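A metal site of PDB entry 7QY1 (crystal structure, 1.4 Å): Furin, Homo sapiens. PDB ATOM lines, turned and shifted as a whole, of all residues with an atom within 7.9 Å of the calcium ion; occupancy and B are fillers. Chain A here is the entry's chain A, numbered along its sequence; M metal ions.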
ATOM      1  N   PRO A   6       4.354  -6.355  22.595  1.00  0.00           N
ATOM      2  CA  PRO A   6       5.095  -6.983  23.690  1.00  0.00           C
ATOM      3  C   PRO A   6       5.553  -5.968  24.720  1.00  0.00           C
ATOM      4  O   PRO A   6       5.870  -4.813  24.391  1.00  0.00           O
ATOM      5  CB  PRO A   6       6.301  -7.611  22.982  1.00  0.00           C
ATOM      6  CG  PRO A   6       5.795  -7.900  21.597  1.00  0.00           C
ATOM      7  CD  PRO A   6       4.886  -6.741  21.274  1.00  0.00           C
ATOM      8  N   THR A   7       5.590  -6.420  25.964  1.00  0.00           N
ATOM      9  CA  THR A   7       5.988  -5.612  27.104  1.00  0.00           C
ATOM     10  C   THR A   7       7.428  -5.845  27.517  1.00  0.00           C
ATOM     11  O   THR A   7       7.888  -5.231  28.490  1.00  0.00           O
ATOM     12  CB  THR A   7       5.067  -5.930  28.281  1.00  0.00           C
ATOM     13  OG1 THR A   7       5.180  -7.328  28.566  1.00  0.00           O
ATOM     14  CG2 THR A   7       3.604  -5.566  27.944  1.00  0.00           C
ATOM     15  N   ASP A   8       8.161  -6.691  26.802  1.00  0.00           N
ATOM     16  CA  ASP A   8       9.520  -7.046  27.204  1.00  0.00           C
ATOM     17  C   ASP A   8      10.402  -5.807  27.309  1.00  0.00           C
ATOM     18  O   ASP A   8      10.260  -4.848  26.548  1.00  0.00           O
ATOM     19  CB  ASP A   8      10.105  -8.036  26.207  1.00  0.00           C
ATOM     20  CG  ASP A   8       9.254  -9.278  26.067  1.00  0.00           C
ATOM     21  OD1 ASP A   8       8.104  -9.125  25.595  1.00  0.00           O
ATOM     22  OD2 ASP A   8       9.714 -10.375  26.444  1.00  0.00           O
ATOM     23  N   PRO A   9      11.347  -5.809  28.248  1.00  0.00           N
ATOM     24  CA  PRO A   9      12.081  -4.570  28.555  1.00  0.00           C
ATOM     25  C   PRO A   9      12.892  -4.044  27.388  1.00  0.00           C
ATOM     26  O   PRO A   9      13.054  -2.825  27.273  1.00  0.00           O
ATOM     27  CB  PRO A   9      12.972  -4.958  29.740  1.00  0.00           C
ATOM     28  CG  PRO A   9      13.017  -6.467  29.731  1.00  0.00           C
ATOM     29  CD  PRO A   9      11.694  -6.909  29.176  1.00  0.00           C
ATOM     30  N   LYS A  10      13.390  -4.907  26.509  1.00  0.00           N
ATOM     31  CA  LYS A  10      14.198  -4.444  25.384  1.00  0.00           C
ATOM     32  C   LYS A  10      13.444  -4.410  24.076  1.00  0.00           C
ATOM     33  O   LYS A  10      14.046  -4.142  23.036  1.00  0.00           O
ATOM     34  CB  LYS A  10      15.452  -5.292  25.244  1.00  0.00           C
ATOM     35  CG  LYS A  10      16.222  -5.257  26.537  1.00  0.00           C
ATOM     36  CD  LYS A  10      17.513  -5.957  26.373  1.00  0.00           C
ATOM     37  CE  LYS A  10      18.647  -5.046  25.956  1.00  0.00           C
ATOM     38  NZ  LYS A  10      18.966  -4.057  27.014  1.00  0.00           N
ATOM     39  N   PHE A  11      12.141  -4.681  24.090  1.00  0.00           N
ATOM     40  CA  PHE A  11      11.389  -4.592  22.837  1.00  0.00           C
ATOM     41  C   PHE A  11      11.479  -3.214  22.210  1.00  0.00           C
ATOM     42  O   PHE A  11      11.625  -3.141  20.972  1.00  0.00           O
ATOM     43  CB  PHE A  11       9.939  -5.020  23.031  1.00  0.00           C
ATOM     44  CG  PHE A  11       9.113  -4.846  21.803  1.00  0.00           C
ATOM     45  CD1 PHE A  11       9.351  -5.626  20.700  1.00  0.00           C
ATOM     46  CD2 PHE A  11       8.089  -3.902  21.750  1.00  0.00           C
ATOM     47  CE1 PHE A  11       8.594  -5.470  19.553  1.00  0.00           C
ATOM     48  CE2 PHE A  11       7.334  -3.743  20.613  1.00  0.00           C
ATOM     49  CZ  PHE A  11       7.591  -4.527  19.519  1.00  0.00           C
ATOM     50  N   GLN A  14      14.282  -3.036  19.860  1.00  0.00           N
ATOM     51  CA  GLN A  14      14.244  -3.856  18.640  1.00  0.00           C
ATOM     52  C   GLN A  14      13.609  -3.044  17.510  1.00  0.00           C
ATOM     53  O   GLN A  14      12.499  -3.304  17.045  1.00  0.00           O
ATOM     54  CB  GLN A  14      13.520  -5.167  18.920  1.00  0.00           C
ATOM     55  CG  GLN A  14      14.254  -5.973  19.991  1.00  0.00           C
ATOM     56  CD  GLN A  14      13.617  -7.309  20.320  1.00  0.00           C
ATOM     57  OE1 GLN A  14      12.467  -7.370  20.731  1.00  0.00           O
ATOM     58  NE2 GLN A  14      14.360  -8.384  20.138  1.00  0.00           N
ATOM     59  N   HIS A  53      18.206 -20.858  28.418  1.00  0.00           N
ATOM     60  CA  HIS A  53      18.160 -19.410  28.502  1.00  0.00           C
ATOM     61  C   HIS A  53      16.752 -18.982  28.934  1.00  0.00           C
ATOM     62  O   HIS A  53      15.769 -19.490  28.406  1.00  0.00           O
ATOM     63  CB  HIS A  53      18.491 -18.785  27.136  1.00  0.00           C
ATOM     64  CG  HIS A  53      18.801 -17.333  27.209  1.00  0.00           C
ATOM     65  ND1 HIS A  53      17.835 -16.388  27.477  1.00  0.00           N
ATOM     66  CD2 HIS A  53      19.963 -16.659  27.090  1.00  0.00           C
ATOM     67  CE1 HIS A  53      18.388 -15.191  27.526  1.00  0.00           C
ATOM     68  NE2 HIS A  53      19.679 -15.324  27.289  1.00  0.00           N
ATOM     69  N   PRO A  54      16.630 -18.072  29.902  1.00  0.00           N
ATOM     70  CA  PRO A  54      15.278 -17.666  30.333  1.00  0.00           C
ATOM     71  C   PRO A  54      14.382 -17.158  29.216  1.00  0.00           C
ATOM     72  O   PRO A  54      13.149 -17.176  29.390  1.00  0.00           O
ATOM     73  CB  PRO A  54      15.566 -16.566  31.380  1.00  0.00           C
ATOM     74  CG  PRO A  54      16.913 -16.872  31.895  1.00  0.00           C
ATOM     75  CD  PRO A  54      17.689 -17.462  30.736  1.00  0.00           C
ATOM     76  N   ASP A  55      14.927 -16.678  28.102  1.00  0.00           N
ATOM     77  CA  ASP A  55      14.108 -16.193  27.003  1.00  0.00           C
ATOM     78  C   ASP A  55      13.944 -17.223  25.882  1.00  0.00           C
ATOM     79  O   ASP A  55      13.277 -16.927  24.888  1.00  0.00           O
ATOM     80  CB  ASP A  55      14.636 -14.879  26.420  1.00  0.00           C
ATOM     81  CG  ASP A  55      13.537 -13.824  26.255  1.00  0.00           C
ATOM     82  OD1 ASP A  55      12.491 -13.928  26.920  1.00  0.00           O
ATOM     83  OD2 ASP A  55      13.717 -12.865  25.469  1.00  0.00           O
ATOM     84  N   LEU A  56      14.548 -18.412  26.025  1.00  0.00           N
ATOM     85  CA  LEU A  56      14.389 -19.490  25.048  1.00  0.00           C
ATOM     86  C   LEU A  56      13.716 -20.733  25.607  1.00  0.00           C
ATOM     87  O   LEU A  56      13.046 -21.450  24.859  1.00  0.00           O
ATOM     88  CB  LEU A  56      15.738 -19.926  24.478  1.00  0.00           C
ATOM     89  CG  LEU A  56      16.539 -18.816  23.796  1.00  0.00           C
ATOM     90  CD1 LEU A  56      17.882 -19.406  23.353  1.00  0.00           C
ATOM     91  CD2 LEU A  56      15.791 -18.205  22.623  1.00  0.00           C
ATOM     92  N   ALA A  96      12.833 -16.645  17.955  1.00  0.00           N
ATOM     93  CA  ALA A  96      11.801 -17.176  18.827  1.00  0.00           C
ATOM     94  C   ALA A  96      11.993 -16.896  20.313  1.00  0.00           C
ATOM     95  O   ALA A  96      11.510 -17.671  21.145  1.00  0.00           O
ATOM     96  CB  ALA A  96      11.668 -18.696  18.645  1.00  0.00           C
ATOM     97  N   ALA A  97      12.638 -15.800  20.660  1.00  0.00           N
ATOM     98  CA  ALA A  97      12.644 -15.416  22.074  1.00  0.00           C
ATOM     99  C   ALA A  97      11.218 -15.198  22.569  1.00  0.00           C
ATOM    100  O   ALA A  97      10.370 -14.633  21.873  1.00  0.00           O
ATOM    101  CB  ALA A  97      13.463 -14.149  22.275  1.00  0.00           C
ATOM    102  N   VAL A  98      10.987 -15.648  23.809  1.00  0.00           N
ATOM    103  CA  VAL A  98       9.654 -15.606  24.413  1.00  0.00           C
ATOM    104  C   VAL A  98       9.207 -14.165  24.600  1.00  0.00           C
ATOM    105  O   VAL A  98      10.014 -13.284  24.942  1.00  0.00           O
ATOM    106  CB  VAL A  98       9.730 -16.342  25.758  1.00  0.00           C
ATOM    107  CG1 VAL A  98       8.458 -16.124  26.550  1.00  0.00           C
ATOM    108  CG2 VAL A  98      10.005 -17.834  25.560  1.00  0.00           C
ATOM    109  N   ALA A  99       7.910 -13.930  24.420  1.00  0.00           N
ATOM    110  CA  ALA A  99       7.334 -12.597  24.555  1.00  0.00           C
ATOM    111  C   ALA A  99       6.627 -12.433  25.891  1.00  0.00           C
ATOM    112  O   ALA A  99       6.112 -13.391  26.459  1.00  0.00           O
ATOM    113  CB  ALA A  99       6.312 -12.324  23.439  1.00  0.00           C
ATOM    114  N   ASN A 100       6.593 -11.181  26.390  1.00  0.00           N
ATOM    115  CA  ASN A 100       5.763 -10.810  27.546  1.00  0.00           C
ATOM    116  C   ASN A 100       6.173 -11.542  28.830  1.00  0.00           C
ATOM    117  O   ASN A 100       5.334 -11.807  29.701  1.00  0.00           O
ATOM    118  CB  ASN A 100       4.273 -11.000  27.229  1.00  0.00           C
ATOM    119  CG  ASN A 100       3.820 -10.135  26.066  1.00  0.00           C
ATOM    120  OD1 ASN A 100       4.004  -8.917  26.086  1.00  0.00           O
ATOM    121  ND2 ASN A 100       3.264 -10.747  25.031  1.00  0.00           N
ATOM    122  N   ASN A 101       7.475 -11.790  28.981  1.00  0.00           N
ATOM    123  CA  ASN A 101       8.012 -12.498  30.133  1.00  0.00           C
ATOM    124  C   ASN A 101       9.034 -11.685  30.925  1.00  0.00           C
ATOM    125  O   ASN A 101       9.730 -12.255  31.773  1.00  0.00           O
ATOM    126  CB  ASN A 101       8.624 -13.842  29.688  1.00  0.00           C
ATOM    127  CG  ASN A 101       9.880 -13.667  28.861  1.00  0.00           C
ATOM    128  OD1 ASN A 101      10.106 -12.626  28.243  1.00  0.00           O
ATOM    129  ND2 ASN A 101      10.718 -14.699  28.853  1.00  0.00           N
ATOM    130  N   GLY A 102       9.150 -10.387  30.673  1.00  0.00           N
ATOM    131  CA  GLY A 102      10.047  -9.535  31.439  1.00  0.00           C
ATOM    132  C   GLY A 102      11.520  -9.748  31.180  1.00  0.00           C
ATOM    133  O   GLY A 102      12.344  -9.241  31.955  1.00  0.00           O
ATOM    134  N   VAL A 103      11.879 -10.466  30.124  1.00  0.00           N
ATOM    135  CA  VAL A 103      13.265 -10.790  29.820  1.00  0.00           C
ATOM    136  C   VAL A 103      13.596 -10.329  28.413  1.00  0.00           C
ATOM    137  O   VAL A 103      12.816 -10.587  27.473  1.00  0.00           O
ATOM    138  CB  VAL A 103      13.531 -12.314  29.965  1.00  0.00           C
ATOM    139  CG1 VAL A 103      14.975 -12.626  29.573  1.00  0.00           C
ATOM    140  CG2 VAL A 103      13.198 -12.808  31.372  1.00  0.00           C
ATOM    141  N   CYS A 104      14.756  -9.683  28.251  1.00  0.00           N
ATOM    142  CA  CYS A 104      15.285  -9.267  26.959  1.00  0.00           C
ATOM    143  C   CYS A 104      14.190  -8.696  26.062  1.00  0.00           C
ATOM    144  O   CYS A 104      13.420  -7.831  26.500  1.00  0.00           O
ATOM    145  CB  CYS A 104      16.059 -10.413  26.307  1.00  0.00           C
ATOM    146  SG  CYS A 104      17.485 -11.076  27.272  1.00  0.00           S
ATOM    147  N   GLY A 105      14.131  -9.135  24.802  1.00  0.00           N
ATOM    148  CA  GLY A 105      13.097  -8.681  23.904  1.00  0.00           C
ATOM    149  C   GLY A 105      12.224  -9.832  23.449  1.00  0.00           C
ATOM    150  O   GLY A 105      11.888 -10.698  24.258  1.00  0.00           O
ATOM    151  N   VAL A 106      11.887  -9.889  22.153  1.00  0.00           N
ATOM    152  CA  VAL A 106      11.040 -10.948  21.610  1.00  0.00           C
ATOM    153  C   VAL A 106      11.621 -11.453  20.301  1.00  0.00           C
ATOM    154  O   VAL A 106      12.363 -10.763  19.599  1.00  0.00           O
ATOM    155  CB  VAL A 106       9.589 -10.501  21.350  1.00  0.00           C
ATOM    156  CG1 VAL A 106       9.005  -9.865  22.583  1.00  0.00           C
ATOM    157  CG2 VAL A 106       9.519  -9.542  20.227  1.00  0.00           C
ATOM    158  N   GLY A 107      11.243 -12.665  19.955  1.00  0.00           N
ATOM    159  CA  GLY A 107      11.503 -13.165  18.626  1.00  0.00           C
ATOM    160  C   GLY A 107      10.491 -12.652  17.609  1.00  0.00           C
ATOM    161  O   GLY A 107       9.394 -12.227  17.966  1.00  0.00           O
ATOM    162  N   TYR A 110       7.497 -15.289  18.058  1.00  0.00           N
ATOM    163  CA  TYR A 110       7.727 -15.530  19.479  1.00  0.00           C
ATOM    164  C   TYR A 110       6.899 -16.678  20.039  1.00  0.00           C
ATOM    165  O   TYR A 110       7.092 -17.009  21.220  1.00  0.00           O
ATOM    166  CB  TYR A 110       7.523 -14.225  20.262  1.00  0.00           C
ATOM    167  CG  TYR A 110       6.198 -13.550  20.098  1.00  0.00           C
ATOM    168  CD1 TYR A 110       5.050 -14.093  20.650  1.00  0.00           C
ATOM    169  CD2 TYR A 110       6.099 -12.322  19.454  1.00  0.00           C
ATOM    170  CE1 TYR A 110       3.830 -13.451  20.535  1.00  0.00           C
ATOM    171  CE2 TYR A 110       4.870 -11.674  19.317  1.00  0.00           C
ATOM    172  CZ  TYR A 110       3.742 -12.249  19.866  1.00  0.00           C
ATOM    173  OH  TYR A 110       2.519 -11.616  19.755  1.00  0.00           O
ATOM    174  N   THR A 247      18.909 -12.570  22.669  1.00  0.00           N
ATOM    175  CA  THR A 247      19.436 -13.409  23.739  1.00  0.00           C
ATOM    176  C   THR A 247      20.926 -13.662  23.544  1.00  0.00           C
ATOM    177  O   THR A 247      21.397 -13.776  22.418  1.00  0.00           O
ATOM    178  CB  THR A 247      18.680 -14.740  23.732  1.00  0.00           C
ATOM    179  OG1 THR A 247      18.601 -15.252  22.382  1.00  0.00           O
ATOM    180  CG2 THR A 247      17.285 -14.550  24.211  1.00  0.00           C
ATOM    181  N   CYS A 253      21.335 -10.749  27.830  1.00  0.00           N
ATOM    182  CA  CYS A 253      20.909 -10.136  26.577  1.00  0.00           C
ATOM    183  C   CYS A 253      22.122  -9.479  25.914  1.00  0.00           C
ATOM    184  O   CYS A 253      23.160  -9.242  26.536  1.00  0.00           O
ATOM    185  CB  CYS A 253      19.833  -9.060  26.807  1.00  0.00           C
ATOM    186  SG  CYS A 253      18.509  -9.469  27.988  1.00  0.00           S
HETATM  187 CA    CA M   1      11.404 -11.910  26.217  1.00  0.00          CA
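OD2 of Asp 8 binds the calcium ion (2.3 Å).
O of Val 103 is bound to the calcium ion (2.3 Å).
O of Val 98 binds the calcium ion, at 2.3 Å.
The calcium ion is bound by the backbone carbonyl oxygen (O) of Gly 105 (2.4 Å).
The calcium ion is bound by OD1 of Asp 55 (2.4 Å).
The calcium ion is bound by OD1 of Asn 101 (2.5 Å).
OD2 of Asp 55 binds the calcium ion (2.6 Å).
Six residues have an atom within 4 Å of the calcium ion: Asp 8, Asp 55, Val 98, Asn 101, Val 103 and Gly 105.
Along chain A the residues within 4 Å of the calcium ion span positions 8 to 105.
The nearest printed residue that does not touch the calcium ion is Cys 104 (4.3 Å).
The side-chain carboxylate (OD1) of Asp 8 is in hydrogen-bond range of the backbone NH (N) of Asn 100, at 2.7 Å.
A ring nitrogen (ND1) of His 53 sits at hydrogen-bond distance from the backbone NH (N) of Asp 55.
SG of Cys 253 forms a disulfide with SG of Cys 104 (2.0 Å).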
